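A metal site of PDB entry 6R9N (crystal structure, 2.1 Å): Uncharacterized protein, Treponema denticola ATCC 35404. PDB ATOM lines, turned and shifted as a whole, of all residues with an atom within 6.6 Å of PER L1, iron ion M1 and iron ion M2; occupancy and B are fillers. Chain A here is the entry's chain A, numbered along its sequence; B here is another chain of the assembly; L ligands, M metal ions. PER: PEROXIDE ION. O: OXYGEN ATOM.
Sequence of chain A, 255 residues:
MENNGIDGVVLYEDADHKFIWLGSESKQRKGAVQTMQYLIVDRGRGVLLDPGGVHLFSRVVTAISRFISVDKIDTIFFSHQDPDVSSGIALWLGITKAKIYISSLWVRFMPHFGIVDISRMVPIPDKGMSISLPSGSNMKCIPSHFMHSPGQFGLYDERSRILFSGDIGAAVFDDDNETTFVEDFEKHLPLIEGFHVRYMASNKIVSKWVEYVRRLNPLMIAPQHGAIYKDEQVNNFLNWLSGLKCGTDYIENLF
The side-chain amide oxygen (OE1) of Gln 152 lies within hydrogen-bond range of the backbone NH (N) of Asp 167 (3.3 Å). The backbone NH (N) of Gln 224 lies within hydrogen-bond range of the backbone carbonyl oxygen (O) of Gly 166, at 2.7 Å. A ring nitrogen (ND1) of His 80 sits at hydrogen-bond distance from the side-chain hydroxyl of Ser 79. NE2 of Gln 81 of chain A is in hydrogen-bond range of OD1 of Asp 82 (3.5 Å). NE1 of Trp 106 of chain B sits close to OE1 of Gln 81 of chain B (3.4 Å). The side-chain carboxylate (OD1) of Asp 82 lies within hydrogen-bond range of the side-chain amide nitrogen (NE2) of Gln 81 of chain B, 2.9 Å away.
CZ of Phe 195 touches O1 of PER L1 (3.9 Å). Trp 106 of chain B touches PER L1 (CZ3 to O2, 3.6 Å). CE1 of Phe 109 of chain B touches O1 of PER L1 (3.5 Å). Hydrophobic or aromatic side chains that line PER L1: His 148, Phe 195, Trp 106 of chain B and Phe 109 of chain B. Of the 23 residues printed, 8 come within 4 Å of PER L1.
Four residues have an atom within 4 Å of iron ion M1: His 80, Asp 82, His 148 and Asp 167. The nearest printed residue that does not touch iron ion M1 is Asp 84 (4.3 Å).
Within 4 Å of iron ion M2: Asp 84, Asp 167, Gln 224 and His 225.
Iron ion M1 is bound by the side-chain carboxylate (OD2) of Asp 82, an oxygen (O) of O L2, the side-chain carboxylate (OD2) of Asp 167, a ring nitrogen (NE2) of His 148, an oxygen (O2) of PER L1 and a ring nitrogen (NE2) of His 80. Iron ion M1 has six donor atoms within binding distance.
An oxygen (O) of O L2 binds iron ion M2, 2.1 Å away. Iron ion M2 is bound by OD2 of Asp 84, at 2.2 Å. Iron ion M2 is bound by OD1 of Asp 167 (2.2 Å). Iron ion M2 is bound by NE2 of His 225 (2.2 Å). O1 of PER L1 binds iron ion M2, 2.3 Å away. Iron ion M2 is bound by OE1 of Gln 224, at 2.3 Å. Iron ion M2 has six donor atoms within binding distance.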
ATOM      1  N   THR A  35     -17.840  -0.877 -10.489  1.00  0.00           N
ATOM      2  CA  THR A  35     -18.469  -1.740  -9.505  1.00  0.00           C
ATOM      3  C   THR A  35     -17.445  -2.071  -8.421  1.00  0.00           C
ATOM      4  O   THR A  35     -16.241  -2.046  -8.655  1.00  0.00           O
ATOM      5  CB  THR A  35     -19.007  -3.019 -10.153  1.00  0.00           C
ATOM      6  OG1 THR A  35     -17.914  -3.707 -10.784  1.00  0.00           O
ATOM      7  CG2 THR A  35     -20.054  -2.690 -11.212  1.00  0.00           C
ATOM      8  N   ASP A  50     -21.053  -9.980  -4.695  1.00  0.00           N
ATOM      9  CA  ASP A  50     -21.384  -9.359  -5.982  1.00  0.00           C
ATOM     10  C   ASP A  50     -20.173  -9.294  -6.895  1.00  0.00           C
ATOM     11  O   ASP A  50     -19.664  -8.204  -7.203  1.00  0.00           O
ATOM     12  CB  ASP A  50     -21.975  -7.969  -5.770  1.00  0.00           C
ATOM     13  CG  ASP A  50     -23.427  -8.021  -5.341  1.00  0.00           C
ATOM     14  OD1 ASP A  50     -23.884  -9.123  -4.931  1.00  0.00           O
ATOM     15  OD2 ASP A  50     -24.120  -6.970  -5.413  1.00  0.00           O
ATOM     16  N   SER A  79     -26.479  -9.651  -4.406  1.00  0.00           N
ATOM     17  CA  SER A  79     -27.467  -8.775  -3.800  1.00  0.00           C
ATOM     18  C   SER A  79     -28.786  -8.810  -4.582  1.00  0.00           C
ATOM     19  O   SER A  79     -29.871  -8.752  -3.986  1.00  0.00           O
ATOM     20  CB  SER A  79     -26.937  -7.340  -3.701  1.00  0.00           C
ATOM     21  OG  SER A  79     -26.663  -6.784  -4.982  1.00  0.00           O
ATOM     22  N   HIS A  80     -28.722  -8.920  -5.913  1.00  0.00           N
ATOM     23  CA  HIS A  80     -29.938  -9.018  -6.737  1.00  0.00           C
ATOM     24  C   HIS A  80     -29.539  -9.509  -8.128  1.00  0.00           C
ATOM     25  O   HIS A  80     -28.446 -10.049  -8.314  1.00  0.00           O
ATOM     26  CB  HIS A  80     -30.697  -7.668  -6.763  1.00  0.00           C
ATOM     27  CG  HIS A  80     -29.917  -6.532  -7.328  1.00  0.00           C
ATOM     28  ND1 HIS A  80     -28.710  -6.102  -6.791  1.00  0.00           N
ATOM     29  CD2 HIS A  80     -30.162  -5.706  -8.372  1.00  0.00           C
ATOM     30  CE1 HIS A  80     -28.265  -5.063  -7.477  1.00  0.00           C
ATOM     31  NE2 HIS A  80     -29.128  -4.814  -8.456  1.00  0.00           N
ATOM     32  N   GLN A  81     -30.404  -9.291  -9.118  1.00  0.00           N
ATOM     33  CA  GLN A  81     -30.345  -9.973 -10.412  1.00  0.00           C
ATOM     34  C   GLN A  81     -29.576  -9.216 -11.487  1.00  0.00           C
ATOM     35  O   GLN A  81     -29.346  -9.780 -12.558  1.00  0.00           O
ATOM     36  CB  GLN A  81     -31.768 -10.243 -10.927  1.00  0.00           C
ATOM     37  CG  GLN A  81     -32.420  -9.067 -11.702  1.00  0.00           C
ATOM     38  CD  GLN A  81     -32.990  -7.984 -10.780  1.00  0.00           C
ATOM     39  OE1 GLN A  81     -32.715  -7.977  -9.559  1.00  0.00           O
ATOM     40  NE2 GLN A  81     -33.786  -7.053 -11.358  1.00  0.00           N
ATOM     41  N   ASP A  82     -29.166  -7.975 -11.228  1.00  0.00           N
ATOM     42  CA  ASP A  82     -28.662  -7.112 -12.282  1.00  0.00           C
ATOM     43  C   ASP A  82     -27.366  -7.647 -12.919  1.00  0.00           C
ATOM     44  O   ASP A  82     -26.578  -8.328 -12.260  1.00  0.00           O
ATOM     45  CB  ASP A  82     -28.409  -5.706 -11.748  1.00  0.00           C
ATOM     46  CG  ASP A  82     -29.654  -4.912 -11.648  1.00  0.00           C
ATOM     47  OD1 ASP A  82     -30.736  -5.460 -11.966  1.00  0.00           O
ATOM     48  OD2 ASP A  82     -29.554  -3.736 -11.272  1.00  0.00           O
ATOM     49  N   ASP A  84     -24.588  -6.021 -13.652  1.00  0.00           N
ATOM     50  CA  ASP A  84     -23.380  -5.604 -12.947  1.00  0.00           C
ATOM     51  C   ASP A  84     -23.118  -6.410 -11.673  1.00  0.00           C
ATOM     52  O   ASP A  84     -22.025  -6.307 -11.106  1.00  0.00           O
ATOM     53  CB  ASP A  84     -23.430  -4.100 -12.650  1.00  0.00           C
ATOM     54  CG  ASP A  84     -24.599  -3.713 -11.755  1.00  0.00           C
ATOM     55  OD1 ASP A  84     -25.696  -4.270 -11.953  1.00  0.00           O
ATOM     56  OD2 ASP A  84     -24.451  -2.857 -10.857  1.00  0.00           O
ATOM     57  N   VAL A  85     -24.081  -7.198 -11.208  1.00  0.00           N
ATOM     58  CA  VAL A  85     -23.926  -8.063 -10.038  1.00  0.00           C
ATOM     59  C   VAL A  85     -23.503  -9.470 -10.432  1.00  0.00           C
ATOM     60  O   VAL A  85     -22.638 -10.071  -9.791  1.00  0.00           O
ATOM     61  CB  VAL A  85     -25.232  -8.116  -9.212  1.00  0.00           C
ATOM     62  CG1 VAL A  85     -25.142  -9.195  -8.116  1.00  0.00           C
ATOM     63  CG2 VAL A  85     -25.565  -6.770  -8.604  1.00  0.00           C
ATOM     64  N   HIS A 148     -33.160  -1.027  -5.692  1.00  0.00           N
ATOM     65  CA  HIS A 148     -34.358  -0.922  -6.548  1.00  0.00           C
ATOM     66  C   HIS A 148     -35.070  -2.249  -6.794  1.00  0.00           C
ATOM     67  O   HIS A 148     -36.283  -2.271  -7.065  1.00  0.00           O
ATOM     68  CB  HIS A 148     -33.960  -0.364  -7.911  1.00  0.00           C
ATOM     69  CG  HIS A 148     -32.886  -1.166  -8.591  1.00  0.00           C
ATOM     70  ND1 HIS A 148     -33.165  -2.174  -9.486  1.00  0.00           N
ATOM     71  CD2 HIS A 148     -31.545  -1.116  -8.483  1.00  0.00           C
ATOM     72  CE1 HIS A 148     -32.042  -2.705  -9.920  1.00  0.00           C
ATOM     73  NE2 HIS A 148     -31.033  -2.083  -9.325  1.00  0.00           N
ATOM     74  N   SER A 149     -34.334  -3.350  -6.726  1.00  0.00           N
ATOM     75  CA  SER A 149     -34.908  -4.594  -7.232  1.00  0.00           C
ATOM     76  C   SER A 149     -35.917  -5.167  -6.243  1.00  0.00           C
ATOM     77  O   SER A 149     -35.713  -5.074  -5.027  1.00  0.00           O
ATOM     78  CB  SER A 149     -33.794  -5.628  -7.486  1.00  0.00           C
ATOM     79  OG  SER A 149     -34.302  -6.941  -7.580  1.00  0.00           O
ATOM     80  N   GLN A 152     -33.911  -7.994  -3.348  1.00  0.00           N
ATOM     81  CA  GLN A 152     -32.541  -7.568  -3.102  1.00  0.00           C
ATOM     82  C   GLN A 152     -32.225  -7.744  -1.633  1.00  0.00           C
ATOM     83  O   GLN A 152     -33.067  -7.453  -0.779  1.00  0.00           O
ATOM     84  CB  GLN A 152     -32.301  -6.080  -3.492  1.00  0.00           C
ATOM     85  CG  GLN A 152     -30.874  -5.574  -3.123  1.00  0.00           C
ATOM     86  CD  GLN A 152     -30.586  -4.092  -3.469  1.00  0.00           C
ATOM     87  OE1 GLN A 152     -29.590  -3.778  -4.139  1.00  0.00           O
ATOM     88  NE2 GLN A 152     -31.410  -3.195  -2.969  1.00  0.00           N
ATOM     89  N   GLY A 166     -25.379  -3.463  -1.416  1.00  0.00           N
ATOM     90  CA  GLY A 166     -25.846  -3.539  -2.782  1.00  0.00           C
ATOM     91  C   GLY A 166     -25.856  -2.164  -3.436  1.00  0.00           C
ATOM     92  O   GLY A 166     -24.898  -1.409  -3.330  1.00  0.00           O
ATOM     93  N   ASP A 167     -26.945  -1.854  -4.139  1.00  0.00           N
ATOM     94  CA  ASP A 167     -27.055  -0.542  -4.787  1.00  0.00           C
ATOM     95  C   ASP A 167     -27.315   0.588  -3.793  1.00  0.00           C
ATOM     96  O   ASP A 167     -27.280   1.761  -4.189  1.00  0.00           O
ATOM     97  CB  ASP A 167     -28.173  -0.540  -5.830  1.00  0.00           C
ATOM     98  CG  ASP A 167     -27.780  -1.243  -7.106  1.00  0.00           C
ATOM     99  OD1 ASP A 167     -26.573  -1.383  -7.381  1.00  0.00           O
ATOM    100  OD2 ASP A 167     -28.703  -1.674  -7.837  1.00  0.00           O
ATOM    101  N   ALA A 170     -24.975   3.650  -3.425  1.00  0.00           N
ATOM    102  CA  ALA A 170     -24.117   3.646  -4.601  1.00  0.00           C
ATOM    103  C   ALA A 170     -23.877   5.061  -5.099  1.00  0.00           C
ATOM    104  O   ALA A 170     -24.783   5.896  -5.137  1.00  0.00           O
ATOM    105  CB  ALA A 170     -24.763   2.821  -5.716  1.00  0.00           C
ATOM    106  N   VAL A 172     -22.631   6.794  -8.660  1.00  0.00           N
ATOM    107  CA  VAL A 172     -22.612   6.381 -10.060  1.00  0.00           C
ATOM    108  C   VAL A 172     -21.685   7.231 -10.918  1.00  0.00           C
ATOM    109  O   VAL A 172     -21.253   6.771 -11.983  1.00  0.00           O
ATOM    110  CB  VAL A 172     -24.060   6.371 -10.612  1.00  0.00           C
ATOM    111  CG1 VAL A 172     -24.107   6.532 -12.132  1.00  0.00           C
ATOM    112  CG2 VAL A 172     -24.772   5.102 -10.167  1.00  0.00           C
ATOM    113  N   PHE A 195     -29.120   9.108  -8.560  1.00  0.00           N
ATOM    114  CA  PHE A 195     -29.342   7.667  -8.553  1.00  0.00           C
ATOM    115  C   PHE A 195     -30.397   7.266  -7.516  1.00  0.00           C
ATOM    116  O   PHE A 195     -31.315   6.493  -7.815  1.00  0.00           O
ATOM    117  CB  PHE A 195     -28.029   6.926  -8.311  1.00  0.00           C
ATOM    118  CG  PHE A 195     -28.165   5.435  -8.322  1.00  0.00           C
ATOM    119  CD1 PHE A 195     -28.176   4.736  -9.524  1.00  0.00           C
ATOM    120  CD2 PHE A 195     -28.265   4.722  -7.134  1.00  0.00           C
ATOM    121  CE1 PHE A 195     -28.274   3.361  -9.548  1.00  0.00           C
ATOM    122  CE2 PHE A 195     -28.407   3.346  -7.144  1.00  0.00           C
ATOM    123  CZ  PHE A 195     -28.402   2.665  -8.346  1.00  0.00           C
ATOM    124  N   TYR A 199     -33.885   5.674  -8.709  1.00  0.00           N
ATOM    125  CA  TYR A 199     -33.899   4.210  -8.668  1.00  0.00           C
ATOM    126  C   TYR A 199     -34.527   3.626  -7.403  1.00  0.00           C
ATOM    127  O   TYR A 199     -35.046   2.507  -7.447  1.00  0.00           O
ATOM    128  CB  TYR A 199     -32.483   3.637  -8.808  1.00  0.00           C
ATOM    129  CG  TYR A 199     -31.785   3.825 -10.144  1.00  0.00           C
ATOM    130  CD1 TYR A 199     -31.402   5.088 -10.589  1.00  0.00           C
ATOM    131  CD2 TYR A 199     -31.456   2.723 -10.929  1.00  0.00           C
ATOM    132  CE1 TYR A 199     -30.734   5.249 -11.805  1.00  0.00           C
ATOM    133  CE2 TYR A 199     -30.794   2.869 -12.144  1.00  0.00           C
ATOM    134  CZ  TYR A 199     -30.435   4.136 -12.572  1.00  0.00           C
ATOM    135  OH  TYR A 199     -29.763   4.272 -13.769  1.00  0.00           O
ATOM    136  N   GLN A 224     -22.213  -1.342  -3.636  1.00  0.00           N
ATOM    137  CA  GLN A 224     -21.766  -2.008  -4.836  1.00  0.00           C
ATOM    138  C   GLN A 224     -21.149  -1.034  -5.848  1.00  0.00           C
ATOM    139  O   GLN A 224     -20.545  -1.481  -6.823  1.00  0.00           O
ATOM    140  CB  GLN A 224     -22.955  -2.780  -5.450  1.00  0.00           C
ATOM    141  CG  GLN A 224     -22.603  -3.891  -6.396  1.00  0.00           C
ATOM    142  CD  GLN A 224     -23.278  -3.711  -7.741  1.00  0.00           C
ATOM    143  OE1 GLN A 224     -24.453  -3.303  -7.805  1.00  0.00           O
ATOM    144  NE2 GLN A 224     -22.544  -3.991  -8.821  1.00  0.00           N
ATOM    145  N   HIS A 225     -21.298   0.277  -5.632  1.00  0.00           N
ATOM    146  CA  HIS A 225     -20.657   1.304  -6.452  1.00  0.00           C
ATOM    147  C   HIS A 225     -20.191   2.453  -5.571  1.00  0.00           C
ATOM    148  O   HIS A 225     -20.965   2.970  -4.773  1.00  0.00           O
ATOM    149  CB  HIS A 225     -21.604   1.879  -7.527  1.00  0.00           C
ATOM    150  CG  HIS A 225     -22.408   0.859  -8.265  1.00  0.00           C
ATOM    151  ND1 HIS A 225     -21.957   0.225  -9.403  1.00  0.00           N
ATOM    152  CD2 HIS A 225     -23.660   0.384  -8.049  1.00  0.00           C
ATOM    153  CE1 HIS A 225     -22.874  -0.610  -9.839  1.00  0.00           C
ATOM    154  NE2 HIS A 225     -23.918  -0.536  -9.030  1.00  0.00           N
ATOM    155  N   GLN B  81     -33.440  -4.481 -17.719  1.00  0.00           N
ATOM    156  CA  GLN B  81     -32.043  -4.887 -17.613  1.00  0.00           C
ATOM    157  C   GLN B  81     -31.851  -6.364 -17.302  1.00  0.00           C
ATOM    158  O   GLN B  81     -30.729  -6.851 -17.409  1.00  0.00           O
ATOM    159  CB  GLN B  81     -31.355  -4.061 -16.513  1.00  0.00           C
ATOM    160  CG  GLN B  81     -31.614  -4.587 -15.082  1.00  0.00           C
ATOM    161  CD  GLN B  81     -32.979  -4.188 -14.536  1.00  0.00           C
ATOM    162  OE1 GLN B  81     -33.879  -3.707 -15.256  1.00  0.00           O
ATOM    163  NE2 GLN B  81     -33.131  -4.356 -13.225  1.00  0.00           N
ATOM    164  N   LEU B 105     -31.698   4.473 -17.885  1.00  0.00           N
ATOM    165  CA  LEU B 105     -31.223   4.017 -16.578  1.00  0.00           C
ATOM    166  C   LEU B 105     -30.192   2.911 -16.694  1.00  0.00           C
ATOM    167  O   LEU B 105     -29.377   2.724 -15.780  1.00  0.00           O
ATOM    168  CB  LEU B 105     -32.394   3.545 -15.717  1.00  0.00           C
ATOM    169  CG  LEU B 105     -33.060   4.549 -14.787  1.00  0.00           C
ATOM    170  CD1 LEU B 105     -33.831   5.586 -15.588  1.00  0.00           C
ATOM    171  CD2 LEU B 105     -34.014   3.846 -13.826  1.00  0.00           C
ATOM    172  N   TRP B 106     -30.222   2.136 -17.776  1.00  0.00           N
ATOM    173  CA  TRP B 106     -29.455   0.914 -17.892  1.00  0.00           C
ATOM    174  C   TRP B 106     -28.311   0.966 -18.901  1.00  0.00           C
ATOM    175  O   TRP B 106     -27.506   0.033 -18.946  1.00  0.00           O
ATOM    176  CB  TRP B 106     -30.387  -0.256 -18.246  1.00  0.00           C
ATOM    177  CG  TRP B 106     -31.492  -0.407 -17.278  1.00  0.00           C
ATOM    178  CD1 TRP B 106     -32.821  -0.418 -17.546  1.00  0.00           C
ATOM    179  CD2 TRP B 106     -31.372  -0.553 -15.864  1.00  0.00           C
ATOM    180  NE1 TRP B 106     -33.547  -0.564 -16.392  1.00  0.00           N
ATOM    181  CE2 TRP B 106     -32.671  -0.646 -15.335  1.00  0.00           C
ATOM    182  CE3 TRP B 106     -30.289  -0.622 -14.985  1.00  0.00           C
ATOM    183  CZ2 TRP B 106     -32.926  -0.800 -13.971  1.00  0.00           C
ATOM    184  CZ3 TRP B 106     -30.529  -0.745 -13.636  1.00  0.00           C
ATOM    185  CH2 TRP B 106     -31.834  -0.843 -13.136  1.00  0.00           C
ATOM    186  N   PHE B 109     -24.885   0.220 -17.620  1.00  0.00           N
ATOM    187  CA  PHE B 109     -24.771  -0.928 -16.744  1.00  0.00           C
ATOM    188  C   PHE B 109     -24.795  -2.262 -17.501  1.00  0.00           C
ATOM    189  O   PHE B 109     -24.891  -3.312 -16.854  1.00  0.00           O
ATOM    190  CB  PHE B 109     -25.899  -0.929 -15.709  1.00  0.00           C
ATOM    191  CG  PHE B 109     -25.842   0.219 -14.718  1.00  0.00           C
ATOM    192  CD1 PHE B 109     -25.089   0.130 -13.572  1.00  0.00           C
ATOM    193  CD2 PHE B 109     -26.602   1.369 -14.925  1.00  0.00           C
ATOM    194  CE1 PHE B 109     -25.052   1.183 -12.654  1.00  0.00           C
ATOM    195  CE2 PHE B 109     -26.579   2.403 -14.021  1.00  0.00           C
ATOM    196  CZ  PHE B 109     -25.805   2.310 -12.879  1.00  0.00           C
HETATM  197  O1  PER L   1     -27.007  -0.432 -10.307  1.00  0.00           O
HETATM  198  O2  PER L   1     -28.414  -0.764 -10.669  1.00  0.00           O
HETATM  199  O     O L   2     -26.993  -3.412  -9.810  1.00  0.00           O
HETATM  200 FE    FE M   1     -28.958  -2.732  -9.622  1.00  0.00          FE
HETATM  201 FE    FE M   2     -25.625  -1.947  -9.276  1.00  0.00          FE
